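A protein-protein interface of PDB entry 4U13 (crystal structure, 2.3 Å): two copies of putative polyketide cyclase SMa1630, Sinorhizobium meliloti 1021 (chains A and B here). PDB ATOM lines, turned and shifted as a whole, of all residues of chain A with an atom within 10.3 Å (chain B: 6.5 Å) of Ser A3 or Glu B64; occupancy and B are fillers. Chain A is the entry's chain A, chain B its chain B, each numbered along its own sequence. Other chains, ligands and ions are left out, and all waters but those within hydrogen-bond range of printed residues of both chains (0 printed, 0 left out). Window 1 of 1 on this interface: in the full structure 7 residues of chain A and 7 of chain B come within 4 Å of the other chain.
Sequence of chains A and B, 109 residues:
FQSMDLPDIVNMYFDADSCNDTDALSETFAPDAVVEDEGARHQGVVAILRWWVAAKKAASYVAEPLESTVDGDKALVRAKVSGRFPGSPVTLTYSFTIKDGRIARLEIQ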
ATOM      1  N   PHE A   1     -25.976 -23.577 -23.641  1.00  0.00           N
ATOM      2  CA  PHE A   1     -24.807 -24.430 -24.025  1.00  0.00           C
ATOM      3  C   PHE A   1     -23.871 -23.795 -25.106  1.00  0.00           C
ATOM      4  O   PHE A   1     -24.294 -23.021 -25.969  1.00  0.00           O
ATOM      5  CB  PHE A   1     -25.271 -25.841 -24.457  1.00  0.00           C
ATOM      6  CG  PHE A   1     -24.252 -26.592 -25.279  1.00  0.00           C
ATOM      7  CD1 PHE A   1     -24.113 -26.336 -26.636  1.00  0.00           C
ATOM      8  CD2 PHE A   1     -23.420 -27.541 -24.690  1.00  0.00           C
ATOM      9  CE1 PHE A   1     -23.148 -26.996 -27.384  1.00  0.00           C
ATOM     10  CE2 PHE A   1     -22.474 -28.231 -25.449  1.00  0.00           C
ATOM     11  CZ  PHE A   1     -22.326 -27.944 -26.787  1.00  0.00           C
ATOM     12  N   GLN A   2     -22.598 -24.174 -25.030  1.00  0.00           N
ATOM     13  CA  GLN A   2     -21.541 -23.614 -25.847  1.00  0.00           C
ATOM     14  C   GLN A   2     -20.462 -24.667 -26.051  1.00  0.00           C
ATOM     15  O   GLN A   2     -20.213 -25.464 -25.159  1.00  0.00           O
ATOM     16  CB  GLN A   2     -20.922 -22.482 -25.059  1.00  0.00           C
ATOM     17  CG  GLN A   2     -20.785 -21.197 -25.813  1.00  0.00           C
ATOM     18  CD  GLN A   2     -20.025 -20.180 -24.995  1.00  0.00           C
ATOM     19  OE1 GLN A   2     -20.023 -20.216 -23.760  1.00  0.00           O
ATOM     20  NE2 GLN A   2     -19.389 -19.262 -25.676  1.00  0.00           N
ATOM     21  N   SER A   3     -19.807 -24.646 -27.205  1.00  0.00           N
ATOM     22  CA  SER A   3     -18.642 -25.508 -27.488  1.00  0.00           C
ATOM     23  C   SER A   3     -17.644 -25.596 -26.349  1.00  0.00           C
ATOM     24  O   SER A   3     -17.266 -26.690 -25.961  1.00  0.00           O
ATOM     25  CB  SER A   3     -17.858 -25.006 -28.699  1.00  0.00           C
ATOM     26  OG  SER A   3     -18.543 -25.312 -29.874  1.00  0.00           O
ATOM     27  N   MET A   4     -17.214 -24.453 -25.819  1.00  0.00           N
ATOM     28  CA  MET A   4     -16.171 -24.453 -24.773  1.00  0.00           C
ATOM     29  C   MET A   4     -16.570 -25.276 -23.550  1.00  0.00           C
ATOM     30  O   MET A   4     -15.708 -25.653 -22.779  1.00  0.00           O
ATOM     31  CB  MET A   4     -15.733 -23.033 -24.419  1.00  0.00           C
ATOM     32  CG  MET A   4     -16.907 -22.148 -24.002  1.00  0.00           C
ATOM     33  SD  MET A   4     -16.384 -20.826 -22.620  1.00  0.00           S
ATOM     34  CE  MET A   4     -17.466 -21.512 -21.108  1.00  0.00           C
ATOM     35  N   ASP A   5     -17.861 -25.600 -23.379  1.00  0.00           N
ATOM     36  CA  ASP A   5     -18.315 -26.483 -22.284  1.00  0.00           C
ATOM     37  C   ASP A   5     -17.843 -27.902 -22.474  1.00  0.00           C
ATOM     38  O   ASP A   5     -17.901 -28.679 -21.533  1.00  0.00           O
ATOM     39  CB  ASP A   5     -19.846 -26.544 -22.156  1.00  0.00           C
ATOM     40  CG  ASP A   5     -20.479 -25.183 -21.895  1.00  0.00           C
ATOM     41  OD1 ASP A   5     -19.747 -24.191 -21.737  1.00  0.00           O
ATOM     42  OD2 ASP A   5     -21.724 -25.093 -21.847  1.00  0.00           O
ATOM     43  N   LEU A   6     -17.412 -28.252 -23.683  1.00  0.00           N
ATOM     44  CA  LEU A   6     -17.014 -29.620 -23.980  1.00  0.00           C
ATOM     45  C   LEU A   6     -15.538 -29.764 -23.813  1.00  0.00           C
ATOM     46  O   LEU A   6     -14.833 -28.812 -24.019  1.00  0.00           O
ATOM     47  CB  LEU A   6     -17.401 -29.966 -25.411  1.00  0.00           C
ATOM     48  CG  LEU A   6     -18.913 -30.085 -25.656  1.00  0.00           C
ATOM     49  CD1 LEU A   6     -19.264 -30.324 -27.123  1.00  0.00           C
ATOM     50  CD2 LEU A   6     -19.460 -31.202 -24.789  1.00  0.00           C
ATOM     51  N   PRO A   7     -15.064 -30.934 -23.371  1.00  0.00           N
ATOM     52  CA  PRO A   7     -13.624 -31.251 -23.462  1.00  0.00           C
ATOM     53  C   PRO A   7     -13.116 -31.089 -24.912  1.00  0.00           C
ATOM     54  O   PRO A   7     -13.840 -31.383 -25.866  1.00  0.00           O
ATOM     55  CB  PRO A   7     -13.537 -32.725 -23.052  1.00  0.00           C
ATOM     56  CG  PRO A   7     -14.813 -33.057 -22.384  1.00  0.00           C
ATOM     57  CD  PRO A   7     -15.843 -32.012 -22.738  1.00  0.00           C
ATOM     58  N   ASP A   8     -11.884 -30.639 -25.101  1.00  0.00           N
ATOM     59  CA  ASP A   8     -11.387 -30.425 -26.461  1.00  0.00           C
ATOM     60  C   ASP A   8     -11.623 -31.624 -27.380  1.00  0.00           C
ATOM     61  O   ASP A   8     -11.943 -31.464 -28.544  1.00  0.00           O
ATOM     62  CB  ASP A   8      -9.894 -30.134 -26.443  1.00  0.00           C
ATOM     63  CG  ASP A   8      -9.595 -28.745 -25.984  1.00  0.00           C
ATOM     64  OD1 ASP A   8     -10.507 -27.901 -26.085  1.00  0.00           O
ATOM     65  OD2 ASP A   8      -8.458 -28.494 -25.527  1.00  0.00           O
ATOM     66  N   ILE A   9     -11.414 -32.820 -26.851  1.00  0.00           N
ATOM     67  CA  ILE A   9     -11.459 -33.999 -27.662  1.00  0.00           C
ATOM     68  C   ILE A   9     -12.884 -34.342 -28.165  1.00  0.00           C
ATOM     69  O   ILE A   9     -13.047 -34.823 -29.277  1.00  0.00           O
ATOM     70  CB  ILE A   9     -10.807 -35.192 -26.947  1.00  0.00           C
ATOM     71  CG1 ILE A   9     -10.537 -36.329 -27.941  1.00  0.00           C
ATOM     72  CG2 ILE A   9     -11.685 -35.679 -25.819  1.00  0.00           C
ATOM     73  CD1 ILE A   9      -9.508 -35.968 -28.995  1.00  0.00           C
ATOM     74  N   VAL A  10     -13.904 -34.104 -27.341  1.00  0.00           N
ATOM     75  CA  VAL A  10     -15.276 -34.311 -27.730  1.00  0.00           C
ATOM     76  C   VAL A  10     -15.605 -33.304 -28.827  1.00  0.00           C
ATOM     77  O   VAL A  10     -16.271 -33.595 -29.832  1.00  0.00           O
ATOM     78  CB  VAL A  10     -16.197 -34.114 -26.539  1.00  0.00           C
ATOM     79  CG1 VAL A  10     -17.645 -34.056 -26.989  1.00  0.00           C
ATOM     80  CG2 VAL A  10     -15.991 -35.241 -25.541  1.00  0.00           C
ATOM     81  N   ASN A  11     -15.142 -32.100 -28.649  1.00  0.00           N
ATOM     82  CA  ASN A  11     -15.346 -31.090 -29.676  1.00  0.00           C
ATOM     83  C   ASN A  11     -14.725 -31.426 -31.049  1.00  0.00           C
ATOM     84  O   ASN A  11     -15.270 -31.082 -32.115  1.00  0.00           O
ATOM     85  CB  ASN A  11     -14.751 -29.823 -29.172  1.00  0.00           C
ATOM     86  CG  ASN A  11     -15.520 -28.647 -29.604  1.00  0.00           C
ATOM     87  OD1 ASN A  11     -16.377 -28.176 -28.853  1.00  0.00           O
ATOM     88  ND2 ASN A  11     -15.240 -28.155 -30.820  1.00  0.00           N
ATOM     89  N   MET A  12     -13.578 -32.093 -31.007  1.00  0.00           N
ATOM     90  CA  MET A  12     -12.912 -32.560 -32.209  1.00  0.00           C
ATOM     91  C   MET A  12     -13.730 -33.629 -32.914  1.00  0.00           C
ATOM     92  O   MET A  12     -13.825 -33.616 -34.132  1.00  0.00           O
ATOM     93  CB  MET A  12     -11.545 -33.079 -31.782  1.00  0.00           C
ATOM     94  CG  MET A  12     -10.618 -33.406 -32.966  1.00  0.00           C
ATOM     95  SD  MET A  12      -8.857 -34.179 -32.342  1.00  0.00           S
ATOM     96  CE  MET A  12      -8.338 -32.664 -31.138  1.00  0.00           C
ATOM     97  N   PHE A  14     -17.061 -33.897 -32.962  1.00  0.00           N
ATOM     98  CA  PHE A  14     -18.203 -33.304 -33.659  1.00  0.00           C
ATOM     99  C   PHE A  14     -17.806 -32.419 -34.809  1.00  0.00           C
ATOM    100  O   PHE A  14     -18.538 -32.338 -35.789  1.00  0.00           O
ATOM    101  CB  PHE A  14     -19.069 -32.504 -32.693  1.00  0.00           C
ATOM    102  CG  PHE A  14     -19.906 -33.385 -31.812  1.00  0.00           C
ATOM    103  CD1 PHE A  14     -20.948 -34.080 -32.345  1.00  0.00           C
ATOM    104  CD2 PHE A  14     -19.597 -33.569 -30.486  1.00  0.00           C
ATOM    105  CE1 PHE A  14     -21.720 -34.904 -31.552  1.00  0.00           C
ATOM    106  CE2 PHE A  14     -20.358 -34.362 -29.690  1.00  0.00           C
ATOM    107  CZ  PHE A  14     -21.411 -35.074 -30.242  1.00  0.00           C
ATOM    108  N   ASP A  15     -16.642 -31.784 -34.730  1.00  0.00           N
ATOM    109  CA  ASP A  15     -16.138 -30.911 -35.846  1.00  0.00           C
ATOM    110  C   ASP A  15     -15.790 -31.754 -37.066  1.00  0.00           C
ATOM    111  O   ASP A  15     -16.083 -31.400 -38.253  1.00  0.00           O
ATOM    112  CB  ASP A  15     -14.873 -30.152 -35.448  1.00  0.00           C
ATOM    113  CG  ASP A  15     -15.147 -28.949 -34.496  1.00  0.00           C
ATOM    114  OD1 ASP A  15     -16.207 -28.299 -34.613  1.00  0.00           O
ATOM    115  OD2 ASP A  15     -14.283 -28.623 -33.640  1.00  0.00           O
ATOM    116  N   ALA A  63     -25.278 -34.199 -36.751  1.00  0.00           N
ATOM    117  CA  ALA A  63     -25.363 -34.244 -35.290  1.00  0.00           C
ATOM    118  C   ALA A  63     -24.976 -32.910 -34.695  1.00  0.00           C
ATOM    119  O   ALA A  63     -23.871 -32.461 -34.854  1.00  0.00           O
ATOM    120  CB  ALA A  63     -24.453 -35.308 -34.723  1.00  0.00           C
ATOM    121  N   GLU A  64     -25.887 -32.269 -33.972  1.00  0.00           N
ATOM    122  CA  GLU A  64     -25.651 -30.939 -33.458  1.00  0.00           C
ATOM    123  C   GLU A  64     -25.695 -30.990 -31.917  1.00  0.00           C
ATOM    124  O   GLU A  64     -26.764 -31.172 -31.369  1.00  0.00           O
ATOM    125  CB  GLU A  64     -26.717 -30.006 -34.038  1.00  0.00           C
ATOM    126  CG  GLU A  64     -26.883 -28.687 -33.295  1.00  0.00           C
ATOM    127  CD  GLU A  64     -28.048 -27.846 -33.807  1.00  0.00           C
ATOM    128  OE1 GLU A  64     -29.050 -28.393 -34.374  1.00  0.00           O
ATOM    129  OE2 GLU A  64     -27.976 -26.617 -33.582  1.00  0.00           O
ATOM    130  N   PRO A  65     -24.543 -30.855 -31.222  1.00  0.00           N
ATOM    131  CA  PRO A  65     -24.610 -30.861 -29.765  1.00  0.00           C
ATOM    132  C   PRO A  65     -25.513 -29.740 -29.213  1.00  0.00           C
ATOM    133  O   PRO A  65     -25.466 -28.613 -29.709  1.00  0.00           O
ATOM    134  CB  PRO A  65     -23.175 -30.632 -29.338  1.00  0.00           C
ATOM    135  CG  PRO A  65     -22.351 -30.931 -30.548  1.00  0.00           C
ATOM    136  CD  PRO A  65     -23.181 -30.601 -31.715  1.00  0.00           C
ATOM    137  N   LEU A  66     -26.369 -30.084 -28.242  1.00  0.00           N
ATOM    138  CA  LEU A  66     -27.307 -29.144 -27.640  1.00  0.00           C
ATOM    139  C   LEU A  66     -26.996 -28.817 -26.178  1.00  0.00           C
ATOM    140  O   LEU A  66     -27.332 -27.754 -25.726  1.00  0.00           O
ATOM    141  CB  LEU A  66     -28.719 -29.726 -27.654  1.00  0.00           C
ATOM    142  CG  LEU A  66     -29.333 -30.009 -29.022  1.00  0.00           C
ATOM    143  CD1 LEU A  66     -30.754 -30.548 -28.838  1.00  0.00           C
ATOM    144  CD2 LEU A  66     -29.298 -28.755 -29.895  1.00  0.00           C
ATOM    145  N   GLU A  67     -26.515 -29.792 -25.422  1.00  0.00           N
ATOM    146  CA  GLU A  67     -26.111 -29.566 -24.058  1.00  0.00           C
ATOM    147  C   GLU A  67     -25.207 -30.646 -23.621  1.00  0.00           C
ATOM    148  O   GLU A  67     -25.056 -31.651 -24.322  1.00  0.00           O
ATOM    149  CB  GLU A  67     -27.283 -29.422 -23.074  1.00  0.00           C
ATOM    150  CG  GLU A  67     -28.471 -30.299 -23.253  1.00  0.00           C
ATOM    151  CD  GLU A  67     -29.523 -29.948 -22.208  1.00  0.00           C
ATOM    152  OE1 GLU A  67     -29.274 -30.247 -21.023  1.00  0.00           O
ATOM    153  OE2 GLU A  67     -30.585 -29.375 -22.552  1.00  0.00           O
ATOM    154  N   SER A  68     -24.562 -30.418 -22.493  1.00  0.00           N
ATOM    155  CA  SER A  68     -23.576 -31.355 -22.013  1.00  0.00           C
ATOM    156  C   SER A  68     -23.362 -31.274 -20.491  1.00  0.00           C
ATOM    157  O   SER A  68     -23.629 -30.256 -19.884  1.00  0.00           O
ATOM    158  CB  SER A  68     -22.261 -31.070 -22.707  1.00  0.00           C
ATOM    159  OG  SER A  68     -21.776 -29.793 -22.307  1.00  0.00           O
ATOM    160  N   THR A  69     -22.904 -32.379 -19.914  1.00  0.00           N
ATOM    161  CA  THR A  69     -22.487 -32.450 -18.529  1.00  0.00           C
ATOM    162  C   THR A  69     -21.250 -33.383 -18.491  1.00  0.00           C
ATOM    163  O   THR A  69     -21.215 -34.404 -19.154  1.00  0.00           O
ATOM    164  CB  THR A  69     -23.628 -32.984 -17.591  1.00  0.00           C
ATOM    165  OG1 THR A  69     -23.898 -34.358 -17.898  1.00  0.00           O
ATOM    166  CG2 THR A  69     -24.947 -32.193 -17.762  1.00  0.00           C
ATOM    167  N   VAL A  70     -20.234 -33.006 -17.735  1.00  0.00           N
ATOM    168  CA  VAL A  70     -19.039 -33.833 -17.590  1.00  0.00           C
ATOM    169  C   VAL A  70     -19.084 -34.424 -16.180  1.00  0.00           C
ATOM    170  O   VAL A  70     -19.461 -33.758 -15.239  1.00  0.00           O
ATOM    171  CB  VAL A  70     -17.728 -33.030 -17.879  1.00  0.00           C
ATOM    172  CG1 VAL A  70     -16.495 -33.944 -17.868  1.00  0.00           C
ATOM    173  CG2 VAL A  70     -17.781 -32.346 -19.253  1.00  0.00           C
ATOM    174  N   ALA A  75     -18.085 -37.851 -20.449  1.00  0.00           N
ATOM    175  CA  ALA A  75     -18.822 -36.691 -20.963  1.00  0.00           C
ATOM    176  C   ALA A  75     -20.064 -37.133 -21.727  1.00  0.00           C
ATOM    177  O   ALA A  75     -20.008 -37.980 -22.626  1.00  0.00           O
ATOM    178  CB  ALA A  75     -17.948 -35.842 -21.845  1.00  0.00           C
ATOM    179  N   VAL A  77     -23.366 -35.949 -23.874  1.00  0.00           N
ATOM    180  CA  VAL A  77     -23.785 -34.904 -24.768  1.00  0.00           C
ATOM    181  C   VAL A  77     -25.108 -35.290 -25.409  1.00  0.00           C
ATOM    182  O   VAL A  77     -25.265 -36.384 -25.955  1.00  0.00           O
ATOM    183  CB  VAL A  77     -22.679 -34.621 -25.840  1.00  0.00           C
ATOM    184  CG1 VAL A  77     -23.051 -33.490 -26.785  1.00  0.00           C
ATOM    185  CG2 VAL A  77     -21.401 -34.202 -25.180  1.00  0.00           C
ATOM    186  N   PHE B  14     -21.915 -20.450 -42.061  1.00  0.00           N
ATOM    187  CA  PHE B  14     -21.128 -20.866 -40.895  1.00  0.00           C
ATOM    188  C   PHE B  14     -20.553 -22.254 -41.041  1.00  0.00           C
ATOM    189  O   PHE B  14     -19.513 -22.531 -40.480  1.00  0.00           O
ATOM    190  CB  PHE B  14     -21.980 -20.803 -39.631  1.00  0.00           C
ATOM    191  CG  PHE B  14     -22.170 -19.406 -39.139  1.00  0.00           C
ATOM    192  CD1 PHE B  14     -21.097 -18.714 -38.572  1.00  0.00           C
ATOM    193  CD2 PHE B  14     -23.368 -18.748 -39.289  1.00  0.00           C
ATOM    194  CE1 PHE B  14     -21.220 -17.414 -38.169  1.00  0.00           C
ATOM    195  CE2 PHE B  14     -23.515 -17.454 -38.836  1.00  0.00           C
ATOM    196  CZ  PHE B  14     -22.432 -16.782 -38.291  1.00  0.00           C
ATOM    197  N   VAL B  62     -12.311 -19.697 -35.178  1.00  0.00           N
ATOM    198  CA  VAL B  62     -13.572 -20.405 -35.150  1.00  0.00           C
ATOM    199  C   VAL B  62     -14.672 -19.357 -34.788  1.00  0.00           C
ATOM    200  O   VAL B  62     -14.576 -18.681 -33.764  1.00  0.00           O
ATOM    201  CB  VAL B  62     -13.431 -21.558 -34.077  1.00  0.00           C
ATOM    202  CG1 VAL B  62     -14.776 -22.079 -33.560  1.00  0.00           C
ATOM    203  CG2 VAL B  62     -12.570 -22.721 -34.601  1.00  0.00           C
ATOM    204  N   ALA B  63     -15.691 -19.215 -35.635  1.00  0.00           N
ATOM    205  CA  ALA B  63     -16.948 -18.475 -35.318  1.00  0.00           C
ATOM    206  C   ALA B  63     -18.111 -19.427 -34.944  1.00  0.00           C
ATOM    207  O   ALA B  63     -18.569 -20.197 -35.750  1.00  0.00           O
ATOM    208  CB  ALA B  63     -17.393 -17.630 -36.484  1.00  0.00           C
ATOM    209  N   GLU B  64     -18.626 -19.329 -33.733  1.00  0.00           N
ATOM    210  CA  GLU B  64     -19.627 -20.271 -33.274  1.00  0.00           C
ATOM    211  C   GLU B  64     -20.939 -19.494 -32.987  1.00  0.00           C
ATOM    212  O   GLU B  64     -20.979 -18.740 -32.033  1.00  0.00           O
ATOM    213  CB  GLU B  64     -19.065 -20.944 -32.016  1.00  0.00           C
ATOM    214  CG  GLU B  64     -20.085 -21.615 -31.127  1.00  0.00           C
ATOM    215  CD  GLU B  64     -19.508 -22.106 -29.807  1.00  0.00           C
ATOM    216  OE1 GLU B  64     -18.494 -21.578 -29.286  1.00  0.00           O
ATOM    217  OE2 GLU B  64     -20.102 -23.034 -29.239  1.00  0.00           O
ATOM    218  N   PRO B  65     -21.999 -19.663 -33.800  1.00  0.00           N
ATOM    219  CA  PRO B  65     -23.250 -18.973 -33.489  1.00  0.00           C
ATOM    220  C   PRO B  65     -23.810 -19.352 -32.109  1.00  0.00           C
ATOM    221  O   PRO B  65     -23.762 -20.523 -31.738  1.00  0.00           O
ATOM    222  CB  PRO B  65     -24.214 -19.452 -34.587  1.00  0.00           C
ATOM    223  CG  PRO B  65     -23.339 -20.040 -35.642  1.00  0.00           C
ATOM    224  CD  PRO B  65     -22.144 -20.572 -34.951  1.00  0.00           C
ATOM    225  N   LEU B  66     -24.278 -18.348 -31.347  1.00  0.00           N
ATOM    226  CA  LEU B  66     -24.780 -18.526 -29.996  1.00  0.00           C
ATOM    227  C   LEU B  66     -26.240 -18.196 -29.857  1.00  0.00           C
ATOM    228  O   LEU B  66     -26.930 -18.772 -29.007  1.00  0.00           O
ATOM    229  CB  LEU B  66     -24.067 -17.594 -29.041  1.00  0.00           C
ATOM    230  CG  LEU B  66     -22.569 -17.795 -28.884  1.00  0.00           C
ATOM    231  CD1 LEU B  66     -22.026 -16.788 -27.845  1.00  0.00           C
ATOM    232  CD2 LEU B  66     -22.239 -19.226 -28.499  1.00  0.00           C
ATOM    233  N   GLU B  67     -26.707 -17.222 -30.623  1.00  0.00           N
ATOM    234  CA  GLU B  67     -28.135 -16.931 -30.683  1.00  0.00           C
ATOM    235  C   GLU B  67     -28.447 -16.129 -31.903  1.00  0.00           C
ATOM    236  O   GLU B  67     -27.532 -15.667 -32.616  1.00  0.00           O
ATOM    237  CB  GLU B  67     -28.646 -16.211 -29.439  1.00  0.00           C
ATOM    238  CG  GLU B  67     -27.791 -15.172 -28.814  1.00  0.00           C
ATOM    239  CD  GLU B  67     -28.462 -14.614 -27.561  1.00  0.00           C
ATOM    240  OE1 GLU B  67     -29.473 -13.902 -27.722  1.00  0.00           O
ATOM    241  OE2 GLU B  67     -27.985 -14.869 -26.424  1.00  0.00           O
ATOM    242  N   VAL B  77     -27.007 -12.496 -35.967  1.00  0.00           N
ATOM    243  CA  VAL B  77     -26.461 -13.631 -35.260  1.00  0.00           C
ATOM    244  C   VAL B  77     -25.320 -13.141 -34.348  1.00  0.00           C
ATOM    245  O   VAL B  77     -24.384 -12.443 -34.799  1.00  0.00           O
ATOM    246  CB  VAL B  77     -25.977 -14.721 -36.284  1.00  0.00           C
ATOM    247  CG1 VAL B  77     -25.416 -15.963 -35.599  1.00  0.00           C
ATOM    248  CG2 VAL B  77     -27.129 -15.205 -37.116  1.00  0.00           C
ATOM    249  N   ARG B  78     -25.400 -13.501 -33.075  1.00  0.00           N
ATOM    250  CA  ARG B  78     -24.287 -13.305 -32.163  1.00  0.00           C
ATOM    251  C   ARG B  78     -23.370 -14.525 -32.244  1.00  0.00           C
ATOM    252  O   ARG B  78     -23.850 -15.678 -32.119  1.00  0.00           O
ATOM    253  CB  ARG B  78     -24.763 -13.114 -30.730  1.00  0.00           C
ATOM    254  CG  ARG B  78     -25.399 -11.768 -30.501  1.00  0.00           C
ATOM    255  CD  ARG B  78     -25.935 -11.718 -29.068  1.00  0.00           C
ATOM    256  NE  ARG B  78     -24.903 -11.901 -28.030  1.00  0.00           N
ATOM    257  CZ  ARG B  78     -24.169 -10.914 -27.514  1.00  0.00           C
ATOM    258  NH1 ARG B  78     -24.336  -9.662 -27.947  1.00  0.00           N
ATOM    259  NH2 ARG B  78     -23.258 -11.166 -26.571  1.00  0.00           N
ATOM    260  N   ALA B  79     -22.076 -14.288 -32.471  1.00  0.00           N
ATOM    261  CA  ALA B  79     -21.184 -15.405 -32.576  1.00  0.00           C
ATOM    262  C   ALA B  79     -19.927 -15.231 -31.751  1.00  0.00           C
ATOM    263  O   ALA B  79     -19.329 -14.160 -31.703  1.00  0.00           O
ATOM    264  CB  ALA B  79     -20.866 -15.689 -34.049  1.00  0.00           C
ATOM    265  N   LYS B  80     -19.511 -16.302 -31.090  1.00  0.00           N
ATOM    266  CA  LYS B  80     -18.279 -16.260 -30.346  1.00  0.00           C
ATOM    267  C   LYS B  80     -17.156 -16.537 -31.353  1.00  0.00           C
ATOM    268  O   LYS B  80     -17.194 -17.522 -32.090  1.00  0.00           O
ATOM    269  CB  LYS B  80     -18.274 -17.277 -29.229  1.00  0.00           C
ATOM    270  CG  LYS B  80     -17.079 -17.169 -28.284  1.00  0.00           C
ATOM    271  CD  LYS B  80     -16.722 -18.536 -27.727  1.00  0.00           C
ATOM    272  CE  LYS B  80     -16.057 -18.441 -26.362  1.00  0.00           C
ATOM    273  NZ  LYS B  80     -15.313 -19.696 -26.070  1.00  0.00           N
ATOM    274  N   VAL B  81     -16.213 -15.610 -31.419  1.00  0.00           N
ATOM    275  CA  VAL B  81     -15.071 -15.725 -32.281  1.00  0.00           C
ATOM    276  C   VAL B  81     -13.807 -15.944 -31.483  1.00  0.00           C
ATOM    277  O   VAL B  81     -13.495 -15.228 -30.592  1.00  0.00           O
ATOM    278  CB  VAL B  81     -14.917 -14.494 -33.151  1.00  0.00           C
ATOM    279  CG1 VAL B  81     -13.762 -14.669 -34.112  1.00  0.00           C
ATOM    280  CG2 VAL B  81     -16.221 -14.274 -33.914  1.00  0.00           C
ATOM    281  N   SER B  82     -13.083 -16.963 -31.836  1.00  0.00           N
ATOM    282  CA  SER B  82     -12.043 -17.461 -30.997  1.00  0.00           C
ATOM    283  C   SER B  82     -10.823 -17.711 -31.903  1.00  0.00           C
ATOM    284  O   SER B  82     -10.990 -18.207 -33.016  1.00  0.00           O
ATOM    285  CB  SER B  82     -12.569 -18.780 -30.440  1.00  0.00           C
ATOM    286  OG  SER B  82     -11.794 -19.192 -29.342  1.00  0.00           O
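N of Ser A3 lies within hydrogen-bond range of OE2 of Glu B64.
The side-chain sulfur (SD) of Met A4 sits close to the side-chain amino group (NZ) of Lys B80 (3.8 Å).
O of Arg B78 lies within hydrogen-bond range of N of Leu B66, at 2.8 Å.
The backbone carbonyl oxygen (O) of Ser A3 lies close to the side-chain amide oxygen (OD1) of Asn A11 (3.4 Å).
The backbone NH (N) of Glu B64 lies within hydrogen-bond range of the backbone carbonyl oxygen (O) of Lys B80 (2.8 Å).
N of Gln A2 lies within hydrogen-bond range of OD2 of Asp A5.
Glu B64 touches Gln A2.
Leu B66 touches Gln A2.
CD of Lys B80 touches NE2 of Gln A2, at 3.4 Å.
Printed residues of chain B within 4 Å of Gln A2: Glu B64, Leu B66 and Lys B80.
Ser A3 touches one residue of chain B.
Of the printed residues of chain B, Met A4 touches Lys B80.
Pro A7 touches none of the printed residues of chain B.
No residue of chain A comes within 4 Å of Ala B63.
Of chain A, only Gln A2 (3.6 Å) and Ser A3 (2.6 Å) come within 4 Å of Glu B64.
No residue of chain A comes within 4 Å of Ala B79.
Of chain A, only Gln A2 and Met A4 come within 4 Å of Lys B80.
Of the 24 printed residues of chain A, 3 touch a printed residue of chain B.
Printed residues of chain A that touch a printed residue of chain B: Gln A2, Ser A3 and Met A4.
Hydrophobic or aromatic side chains of chain A that line the printed part of chain B: Met A4.
Of the 13 printed residues of chain B, 3 touch a printed residue of chain A.
Hydrophobic or aromatic side chains of chain B that line the printed part of chain A: Leu B66.
Among the printed residues, 5 pairs touch across the chains.
Among the printed residues, no Asp or Glu carboxylate lies within 4 Å of a Lys or Arg side-chain nitrogen of the other chain.
Positions printed for both chains: 14, 63, 64, 65, 66, 67 and 77.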
